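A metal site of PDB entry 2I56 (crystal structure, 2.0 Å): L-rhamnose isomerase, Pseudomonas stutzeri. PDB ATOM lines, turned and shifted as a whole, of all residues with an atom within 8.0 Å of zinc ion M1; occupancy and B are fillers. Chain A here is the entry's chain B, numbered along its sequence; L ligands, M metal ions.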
ATOM      1  N   TRP A  57      24.333 -17.085  -1.480  1.00  0.00           N
ATOM      2  CA  TRP A  57      25.746 -17.301  -1.207  1.00  0.00           C
ATOM      3  C   TRP A  57      26.076 -17.257   0.270  1.00  0.00           C
ATOM      4  O   TRP A  57      27.235 -17.381   0.657  1.00  0.00           O
ATOM      5  CB  TRP A  57      26.594 -16.268  -1.966  1.00  0.00           C
ATOM      6  CG  TRP A  57      26.355 -14.849  -1.539  1.00  0.00           C
ATOM      7  CD1 TRP A  57      27.082 -14.134  -0.621  1.00  0.00           C
ATOM      8  CD2 TRP A  57      25.336 -13.964  -2.023  1.00  0.00           C
ATOM      9  NE1 TRP A  57      26.568 -12.862  -0.505  1.00  0.00           N
ATOM     10  CE2 TRP A  57      25.491 -12.733  -1.347  1.00  0.00           C
ATOM     11  CE3 TRP A  57      24.292 -14.098  -2.955  1.00  0.00           C
ATOM     12  CZ2 TRP A  57      24.659 -11.635  -1.577  1.00  0.00           C
ATOM     13  CZ3 TRP A  57      23.453 -12.998  -3.178  1.00  0.00           C
ATOM     14  CH2 TRP A  57      23.645 -11.783  -2.491  1.00  0.00           C
ATOM     15  N   ASN A 127      21.398 -10.325  -8.282  1.00  0.00           N
ATOM     16  CA  ASN A 127      22.696  -9.718  -7.999  1.00  0.00           C
ATOM     17  C   ASN A 127      23.689 -10.029  -9.124  1.00  0.00           C
ATOM     18  O   ASN A 127      23.993 -11.196  -9.379  1.00  0.00           O
ATOM     19  CB  ASN A 127      23.242 -10.258  -6.673  1.00  0.00           C
ATOM     20  CG  ASN A 127      22.523  -9.695  -5.472  1.00  0.00           C
ATOM     21  OD1 ASN A 127      22.854  -8.608  -4.987  1.00  0.00           O
ATOM     22  ND2 ASN A 127      21.513 -10.409  -4.996  1.00  0.00           N
ATOM     23  N   THR A 177      20.413  -5.643  -8.064  1.00  0.00           N
ATOM     24  CA  THR A 177      21.361  -4.968  -7.193  1.00  0.00           C
ATOM     25  C   THR A 177      22.721  -4.966  -7.874  1.00  0.00           C
ATOM     26  O   THR A 177      23.180  -6.009  -8.373  1.00  0.00           O
ATOM     27  CB  THR A 177      21.485  -5.680  -5.837  1.00  0.00           C
ATOM     28  OG1 THR A 177      20.259  -5.533  -5.120  1.00  0.00           O
ATOM     29  CG2 THR A 177      22.620  -5.066  -5.026  1.00  0.00           C
ATOM     30  N   TRP A 179      26.618  -4.120  -7.233  1.00  0.00           N
ATOM     31  CA  TRP A 179      27.775  -3.781  -6.422  1.00  0.00           C
ATOM     32  C   TRP A 179      28.959  -4.207  -7.270  1.00  0.00           C
ATOM     33  O   TRP A 179      29.013  -5.347  -7.726  1.00  0.00           O
ATOM     34  CB  TRP A 179      27.833  -4.564  -5.099  1.00  0.00           C
ATOM     35  CG  TRP A 179      29.149  -4.299  -4.414  1.00  0.00           C
ATOM     36  CD1 TRP A 179      29.528  -3.131  -3.804  1.00  0.00           C
ATOM     37  CD2 TRP A 179      30.310  -5.157  -4.388  1.00  0.00           C
ATOM     38  NE1 TRP A 179      30.844  -3.206  -3.418  1.00  0.00           N
ATOM     39  CE2 TRP A 179      31.346  -4.436  -3.765  1.00  0.00           C
ATOM     40  CE3 TRP A 179      30.560  -6.455  -4.846  1.00  0.00           C
ATOM     41  CZ2 TRP A 179      32.623  -4.967  -3.578  1.00  0.00           C
ATOM     42  CZ3 TRP A 179      31.843  -6.987  -4.666  1.00  0.00           C
ATOM     43  CH2 TRP A 179      32.853  -6.245  -4.031  1.00  0.00           C
ATOM     44  N   GLU A 219      25.006  -0.007  -4.826  1.00  0.00           N
ATOM     45  CA  GLU A 219      25.523  -0.161  -3.476  1.00  0.00           C
ATOM     46  C   GLU A 219      26.907   0.448  -3.307  1.00  0.00           C
ATOM     47  O   GLU A 219      27.851   0.058  -3.999  1.00  0.00           O
ATOM     48  CB  GLU A 219      25.587  -1.659  -3.142  1.00  0.00           C
ATOM     49  CG  GLU A 219      25.818  -1.997  -1.686  1.00  0.00           C
ATOM     50  CD  GLU A 219      25.858  -3.496  -1.460  1.00  0.00           C
ATOM     51  OE1 GLU A 219      25.147  -4.231  -2.177  1.00  0.00           O
ATOM     52  OE2 GLU A 219      26.589  -3.933  -0.555  1.00  0.00           O
ATOM     53  N   HIS A 220      27.030   1.416  -2.392  1.00  0.00           N
ATOM     54  CA  HIS A 220      28.323   2.068  -2.152  1.00  0.00           C
ATOM     55  C   HIS A 220      29.157   1.277  -1.167  1.00  0.00           C
ATOM     56  O   HIS A 220      28.627   0.513  -0.350  1.00  0.00           O
ATOM     57  CB  HIS A 220      28.132   3.489  -1.610  1.00  0.00           C
ATOM     58  CG  HIS A 220      27.358   3.547  -0.332  1.00  0.00           C
ATOM     59  ND1 HIS A 220      25.984   3.598  -0.291  1.00  0.00           N
ATOM     60  CD2 HIS A 220      27.764   3.538   0.964  1.00  0.00           C
ATOM     61  CE1 HIS A 220      25.574   3.624   0.962  1.00  0.00           C
ATOM     62  NE2 HIS A 220      26.643   3.592   1.746  1.00  0.00           N
ATOM     63  N   LYS A 221      30.476   1.466  -1.243  1.00  0.00           N
ATOM     64  CA  LYS A 221      31.399   0.778  -0.350  1.00  0.00           C
ATOM     65  C   LYS A 221      32.677   1.625  -0.309  1.00  0.00           C
ATOM     66  O   LYS A 221      33.215   2.016  -1.341  1.00  0.00           O
ATOM     67  CB  LYS A 221      31.713  -0.623  -0.878  1.00  0.00           C
ATOM     68  CG  LYS A 221      32.442  -1.505   0.127  1.00  0.00           C
ATOM     69  CD  LYS A 221      32.755  -2.875  -0.451  1.00  0.00           C
ATOM     70  CE  LYS A 221      33.373  -3.781   0.608  1.00  0.00           C
ATOM     71  NZ  LYS A 221      33.667  -5.140   0.080  1.00  0.00           N
ATOM     72  N   LEU A 252      21.329   1.287  -1.931  1.00  0.00           N
ATOM     73  CA  LEU A 252      21.327   0.230  -0.923  1.00  0.00           C
ATOM     74  C   LEU A 252      22.387   0.570   0.117  1.00  0.00           C
ATOM     75  O   LEU A 252      23.513   0.912  -0.235  1.00  0.00           O
ATOM     76  CB  LEU A 252      21.670  -1.118  -1.547  1.00  0.00           C
ATOM     77  CG  LEU A 252      20.560  -1.827  -2.327  1.00  0.00           C
ATOM     78  CD1 LEU A 252      21.085  -3.163  -2.823  1.00  0.00           C
ATOM     79  CD2 LEU A 252      19.349  -2.035  -1.431  1.00  0.00           C
ATOM     80  N   VAL A 253      22.016   0.478   1.393  1.00  0.00           N
ATOM     81  CA  VAL A 253      22.948   0.776   2.488  1.00  0.00           C
ATOM     82  C   VAL A 253      23.387  -0.512   3.171  1.00  0.00           C
ATOM     83  O   VAL A 253      22.581  -1.191   3.819  1.00  0.00           O
ATOM     84  CB  VAL A 253      22.287   1.697   3.551  1.00  0.00           C
ATOM     85  CG1 VAL A 253      23.274   1.953   4.681  1.00  0.00           C
ATOM     86  CG2 VAL A 253      21.877   3.014   2.917  1.00  0.00           C
ATOM     87  N   ASP A 254      24.668  -0.859   3.027  1.00  0.00           N
ATOM     88  CA  ASP A 254      25.228  -2.053   3.664  1.00  0.00           C
ATOM     89  C   ASP A 254      25.972  -1.571   4.902  1.00  0.00           C
ATOM     90  O   ASP A 254      26.978  -0.866   4.802  1.00  0.00           O
ATOM     91  CB  ASP A 254      26.192  -2.759   2.699  1.00  0.00           C
ATOM     92  CG  ASP A 254      26.674  -4.093   3.238  1.00  0.00           C
ATOM     93  OD1 ASP A 254      27.216  -4.128   4.361  1.00  0.00           O
ATOM     94  OD2 ASP A 254      26.504  -5.109   2.540  1.00  0.00           O
ATOM     95  N   LEU A 255      25.471  -1.965   6.068  1.00  0.00           N
ATOM     96  CA  LEU A 255      26.033  -1.547   7.358  1.00  0.00           C
ATOM     97  C   LEU A 255      27.559  -1.476   7.462  1.00  0.00           C
ATOM     98  O   LEU A 255      28.097  -0.462   7.895  1.00  0.00           O
ATOM     99  CB  LEU A 255      25.483  -2.461   8.470  1.00  0.00           C
ATOM    100  CG  LEU A 255      25.635  -2.044   9.945  1.00  0.00           C
ATOM    101  CD1 LEU A 255      27.083  -2.168  10.410  1.00  0.00           C
ATOM    102  CD2 LEU A 255      25.111  -0.625  10.129  1.00  0.00           C
ATOM    103  N   GLY A 256      28.253  -2.535   7.049  1.00  0.00           N
ATOM    104  CA  GLY A 256      29.698  -2.546   7.151  1.00  0.00           C
ATOM    105  C   GLY A 256      30.503  -1.885   6.045  1.00  0.00           C
ATOM    106  O   GLY A 256      31.726  -2.065   5.990  1.00  0.00           O
ATOM    107  N   HIS A 257      29.860  -1.120   5.177  1.00  0.00           N
ATOM    108  CA  HIS A 257      30.555  -0.468   4.067  1.00  0.00           C
ATOM    109  C   HIS A 257      30.857   1.007   4.295  1.00  0.00           C
ATOM    110  O   HIS A 257      31.030   1.766   3.336  1.00  0.00           O
ATOM    111  CB  HIS A 257      29.752  -0.579   2.770  1.00  0.00           C
ATOM    112  CG  HIS A 257      29.640  -1.975   2.242  1.00  0.00           C
ATOM    113  ND1 HIS A 257      29.104  -2.254   1.001  1.00  0.00           N
ATOM    114  CD2 HIS A 257      29.996  -3.168   2.769  1.00  0.00           C
ATOM    115  CE1 HIS A 257      29.136  -3.558   0.799  1.00  0.00           C
ATOM    116  NE2 HIS A 257      29.680  -4.139   1.852  1.00  0.00           N
ATOM    117  N   PHE A 280      18.280  -1.955   2.819  1.00  0.00           N
ATOM    118  CA  PHE A 280      19.399  -2.023   3.757  1.00  0.00           C
ATOM    119  C   PHE A 280      19.947  -3.435   3.774  1.00  0.00           C
ATOM    120  O   PHE A 280      19.179  -4.403   3.854  1.00  0.00           O
ATOM    121  CB  PHE A 280      18.919  -1.608   5.149  1.00  0.00           C
ATOM    122  CG  PHE A 280      20.023  -1.301   6.126  1.00  0.00           C
ATOM    123  CD1 PHE A 280      20.708  -2.329   6.774  1.00  0.00           C
ATOM    124  CD2 PHE A 280      20.386   0.013   6.394  1.00  0.00           C
ATOM    125  CE1 PHE A 280      21.747  -2.041   7.679  1.00  0.00           C
ATOM    126  CE2 PHE A 280      21.419   0.317   7.290  1.00  0.00           C
ATOM    127  CZ  PHE A 280      22.100  -0.725   7.938  1.00  0.00           C
ATOM    128  N   HIS A 281      21.265  -3.565   3.658  1.00  0.00           N
ATOM    129  CA  HIS A 281      21.919  -4.866   3.709  1.00  0.00           C
ATOM    130  C   HIS A 281      22.466  -5.042   5.107  1.00  0.00           C
ATOM    131  O   HIS A 281      23.373  -4.324   5.524  1.00  0.00           O
ATOM    132  CB  HIS A 281      23.051  -4.965   2.682  1.00  0.00           C
ATOM    133  CG  HIS A 281      22.594  -5.372   1.321  1.00  0.00           C
ATOM    134  ND1 HIS A 281      23.470  -5.750   0.325  1.00  0.00           N
ATOM    135  CD2 HIS A 281      21.353  -5.474   0.796  1.00  0.00           C
ATOM    136  CE1 HIS A 281      22.781  -6.080  -0.757  1.00  0.00           C
ATOM    137  NE2 HIS A 281      21.498  -5.915  -0.503  1.00  0.00           N
ATOM    138  N   PHE A 282      21.913  -6.003   5.835  1.00  0.00           N
ATOM    139  CA  PHE A 282      22.299  -6.256   7.210  1.00  0.00           C
ATOM    140  C   PHE A 282      23.489  -7.181   7.433  1.00  0.00           C
ATOM    141  O   PHE A 282      23.693  -8.159   6.718  1.00  0.00           O
ATOM    142  CB  PHE A 282      21.091  -6.799   7.976  1.00  0.00           C
ATOM    143  CG  PHE A 282      19.945  -5.822   8.077  1.00  0.00           C
ATOM    144  CD1 PHE A 282      19.984  -4.790   9.010  1.00  0.00           C
ATOM    145  CD2 PHE A 282      18.864  -5.918   7.213  1.00  0.00           C
ATOM    146  CE1 PHE A 282      18.945  -3.861   9.084  1.00  0.00           C
ATOM    147  CE2 PHE A 282      17.818  -4.995   7.281  1.00  0.00           C
ATOM    148  CZ  PHE A 282      17.857  -3.962   8.214  1.00  0.00           C
ATOM    149  N   ASN A 283      24.256  -6.819   8.455  1.00  0.00           N
ATOM    150  CA  ASN A 283      25.436  -7.532   8.914  1.00  0.00           C
ATOM    151  C   ASN A 283      25.985  -6.657  10.030  1.00  0.00           C
ATOM    152  O   ASN A 283      25.422  -5.601  10.331  1.00  0.00           O
ATOM    153  CB  ASN A 283      26.467  -7.692   7.790  1.00  0.00           C
ATOM    154  CG  ASN A 283      26.745  -6.400   7.033  1.00  0.00           C
ATOM    155  OD1 ASN A 283      27.218  -5.415   7.605  1.00  0.00           O
ATOM    156  ND2 ASN A 283      26.463  -6.407   5.732  1.00  0.00           N
ATOM    157  N   ASP A 289      34.635  -4.069   6.510  1.00  0.00           N
ATOM    158  CA  ASP A 289      33.476  -4.782   5.979  1.00  0.00           C
ATOM    159  C   ASP A 289      33.639  -6.218   6.434  1.00  0.00           C
ATOM    160  O   ASP A 289      33.885  -7.111   5.628  1.00  0.00           O
ATOM    161  CB  ASP A 289      33.432  -4.708   4.453  1.00  0.00           C
ATOM    162  CG  ASP A 289      32.255  -5.459   3.871  1.00  0.00           C
ATOM    163  OD1 ASP A 289      31.154  -5.394   4.474  1.00  0.00           O
ATOM    164  OD2 ASP A 289      32.417  -6.104   2.816  1.00  0.00           O
ATOM    165  N   ASP A 291      31.431  -8.257   7.599  1.00  0.00           N
ATOM    166  CA  ASP A 291      30.289  -9.107   7.240  1.00  0.00           C
ATOM    167  C   ASP A 291      29.915 -10.137   8.309  1.00  0.00           C
ATOM    168  O   ASP A 291      29.607 -11.282   7.999  1.00  0.00           O
ATOM    169  CB  ASP A 291      30.569  -9.843   5.913  1.00  0.00           C
ATOM    170  CG  ASP A 291      30.696  -8.897   4.742  1.00  0.00           C
ATOM    171  OD1 ASP A 291      30.029  -7.834   4.775  1.00  0.00           O
ATOM    172  OD2 ASP A 291      31.446  -9.200   3.790  1.00  0.00           O
ATOM    173  N   MET A 325      17.864  -7.180   2.962  1.00  0.00           N
ATOM    174  CA  MET A 325      18.550  -8.450   2.757  1.00  0.00           C
ATOM    175  C   MET A 325      19.719  -8.595   3.717  1.00  0.00           C
ATOM    176  O   MET A 325      20.283  -7.603   4.179  1.00  0.00           O
ATOM    177  CB  MET A 325      19.083  -8.535   1.325  1.00  0.00           C
ATOM    178  CG  MET A 325      19.860  -9.826   1.045  1.00  0.00           C
ATOM    179  SD  MET A 325      20.783  -9.840  -0.522  1.00  0.00           S
ATOM    180  CE  MET A 325      22.448  -9.421   0.068  1.00  0.00           C
ATOM    181  N   ILE A 326      20.068  -9.836   4.025  1.00  0.00           N
ATOM    182  CA  ILE A 326      21.201 -10.096   4.879  1.00  0.00           C
ATOM    183  C   ILE A 326      22.368 -10.328   3.916  1.00  0.00           C
ATOM    184  O   ILE A 326      22.222 -11.034   2.918  1.00  0.00           O
ATOM    185  CB  ILE A 326      20.997 -11.356   5.742  1.00  0.00           C
ATOM    186  CG1 ILE A 326      19.922 -11.104   6.803  1.00  0.00           C
ATOM    187  CG2 ILE A 326      22.326 -11.758   6.396  1.00  0.00           C
ATOM    188  CD1 ILE A 326      19.543 -12.335   7.604  1.00  0.00           C
ATOM    189  N   ASP A 327      23.507  -9.710   4.198  1.00  0.00           N
ATOM    190  CA  ASP A 327      24.688  -9.874   3.359  1.00  0.00           C
ATOM    191  C   ASP A 327      25.829 -10.115   4.342  1.00  0.00           C
ATOM    192  O   ASP A 327      26.455  -9.182   4.849  1.00  0.00           O
ATOM    193  CB  ASP A 327      24.945  -8.620   2.533  1.00  0.00           C
ATOM    194  CG  ASP A 327      26.049  -8.799   1.512  1.00  0.00           C
ATOM    195  OD1 ASP A 327      26.604  -9.921   1.415  1.00  0.00           O
ATOM    196  OD2 ASP A 327      26.372  -7.832   0.801  1.00  0.00           O
ATOM    197  N   GLN A 328      26.089 -11.392   4.629  1.00  0.00           N
ATOM    198  CA  GLN A 328      27.112 -11.756   5.586  1.00  0.00           C
ATOM    199  C   GLN A 328      28.005 -12.885   5.070  1.00  0.00           C
ATOM    200  O   GLN A 328      27.723 -13.521   4.053  1.00  0.00           O
ATOM    201  CB  GLN A 328      26.448 -12.199   6.901  1.00  0.00           C
ATOM    202  CG  GLN A 328      25.649 -11.087   7.593  1.00  0.00           C
ATOM    203  CD  GLN A 328      24.748 -11.593   8.713  1.00  0.00           C
ATOM    204  OE1 GLN A 328      24.070 -10.803   9.384  1.00  0.00           O
ATOM    205  NE2 GLN A 328      24.716 -12.913   8.914  1.00  0.00           N
HETATM  206  C1  LIG L   1      30.532  -6.426  -1.176  1.00  0.00           C
HETATM  207  C2  LIG L   1      29.019  -6.356  -0.993  1.00  0.00           C
HETATM  208  C3  LIG L   1      28.312  -7.089  -2.139  1.00  0.00           C
HETATM  209  C4  LIG L   1      28.782  -8.539  -2.298  1.00  0.00           C
HETATM  210  C5  LIG L   1      27.778  -9.383  -3.086  1.00  0.00           C
HETATM  211  C6  LIG L   1      28.320 -10.784  -3.272  1.00  0.00           C
HETATM  212  O1  LIG L   1      31.277  -6.364  -0.189  1.00  0.00           O
HETATM  213  O2  LIG L   1      28.668  -6.942   0.248  1.00  0.00           O
HETATM  214  O3  LIG L   1      26.905  -7.061  -1.930  1.00  0.00           O
HETATM  215  O4  LIG L   1      29.005  -9.129  -1.029  1.00  0.00           O
HETATM  216  O5  LIG L   1      27.542  -8.797  -4.352  1.00  0.00           O
HETATM  217 ZN    ZN M   1      25.774  -5.699   0.542  1.00  0.00          ZN
HETATM  218 ZN    ZN M   2      29.750  -6.438   2.877  1.00  0.00          ZN
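Zinc ion M1 is bound by OD2 of Asp 254 (2.2 Å), OD2 of Asp 327 (2.2 Å), OE2 of Glu 219 (2.2 Å) and ND1 of His 281 (2.3 Å).
Zinc ion M1 has four donor atoms within binding distance.
A ring nitrogen (NE2) of His 257 sits close to an oxygen (O2) of the ligand (3.4 Å).
An oxygen (O2) of the ligand sits close to the side-chain carboxylate (OD2) of Asp 327, at 2.5 Å.
NZ of Lys 221 lies within hydrogen-bond range of O1 of the ligand, at 2.7 Å.
An oxygen (O3) of the ligand lies within hydrogen-bond range of the side-chain carboxylate (OE1) of Glu 219.
The side-chain amide nitrogen (ND2) of Asn 283 lies within hydrogen-bond range of the side-chain carboxylate (OD1) of Asp 254 (2.8 Å).
The side-chain carboxylate of Glu 219 sits close to a ring nitrogen (ND1) of His 257, 3.4 Å away.
The backbone carbonyl oxygen (O) of Phe 282 sits at hydrogen-bond distance from the backbone NH (N) of Asp 327 (3.0 Å).
N of Gly 256 lies close to OD1 of Asp 254 (3.3 Å).
ND1 of His 257 lies within hydrogen-bond range of O of His 220 (3.1 Å).
The side-chain amide nitrogen of Asn 283 lies within hydrogen-bond range of the backbone carbonyl oxygen of Asp 327 (2.9 Å).
The backbone NH (N) of His 281 sits at hydrogen-bond distance from the backbone carbonyl oxygen (O) of Val 253 (2.7 Å).
O of His 281 sits at hydrogen-bond distance from N of Leu 255.
His 257 touches zinc ion M1.
Within 4 Å of zinc ion M1: Glu 219, Asp 254, His 257, His 281 and Asp 327.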
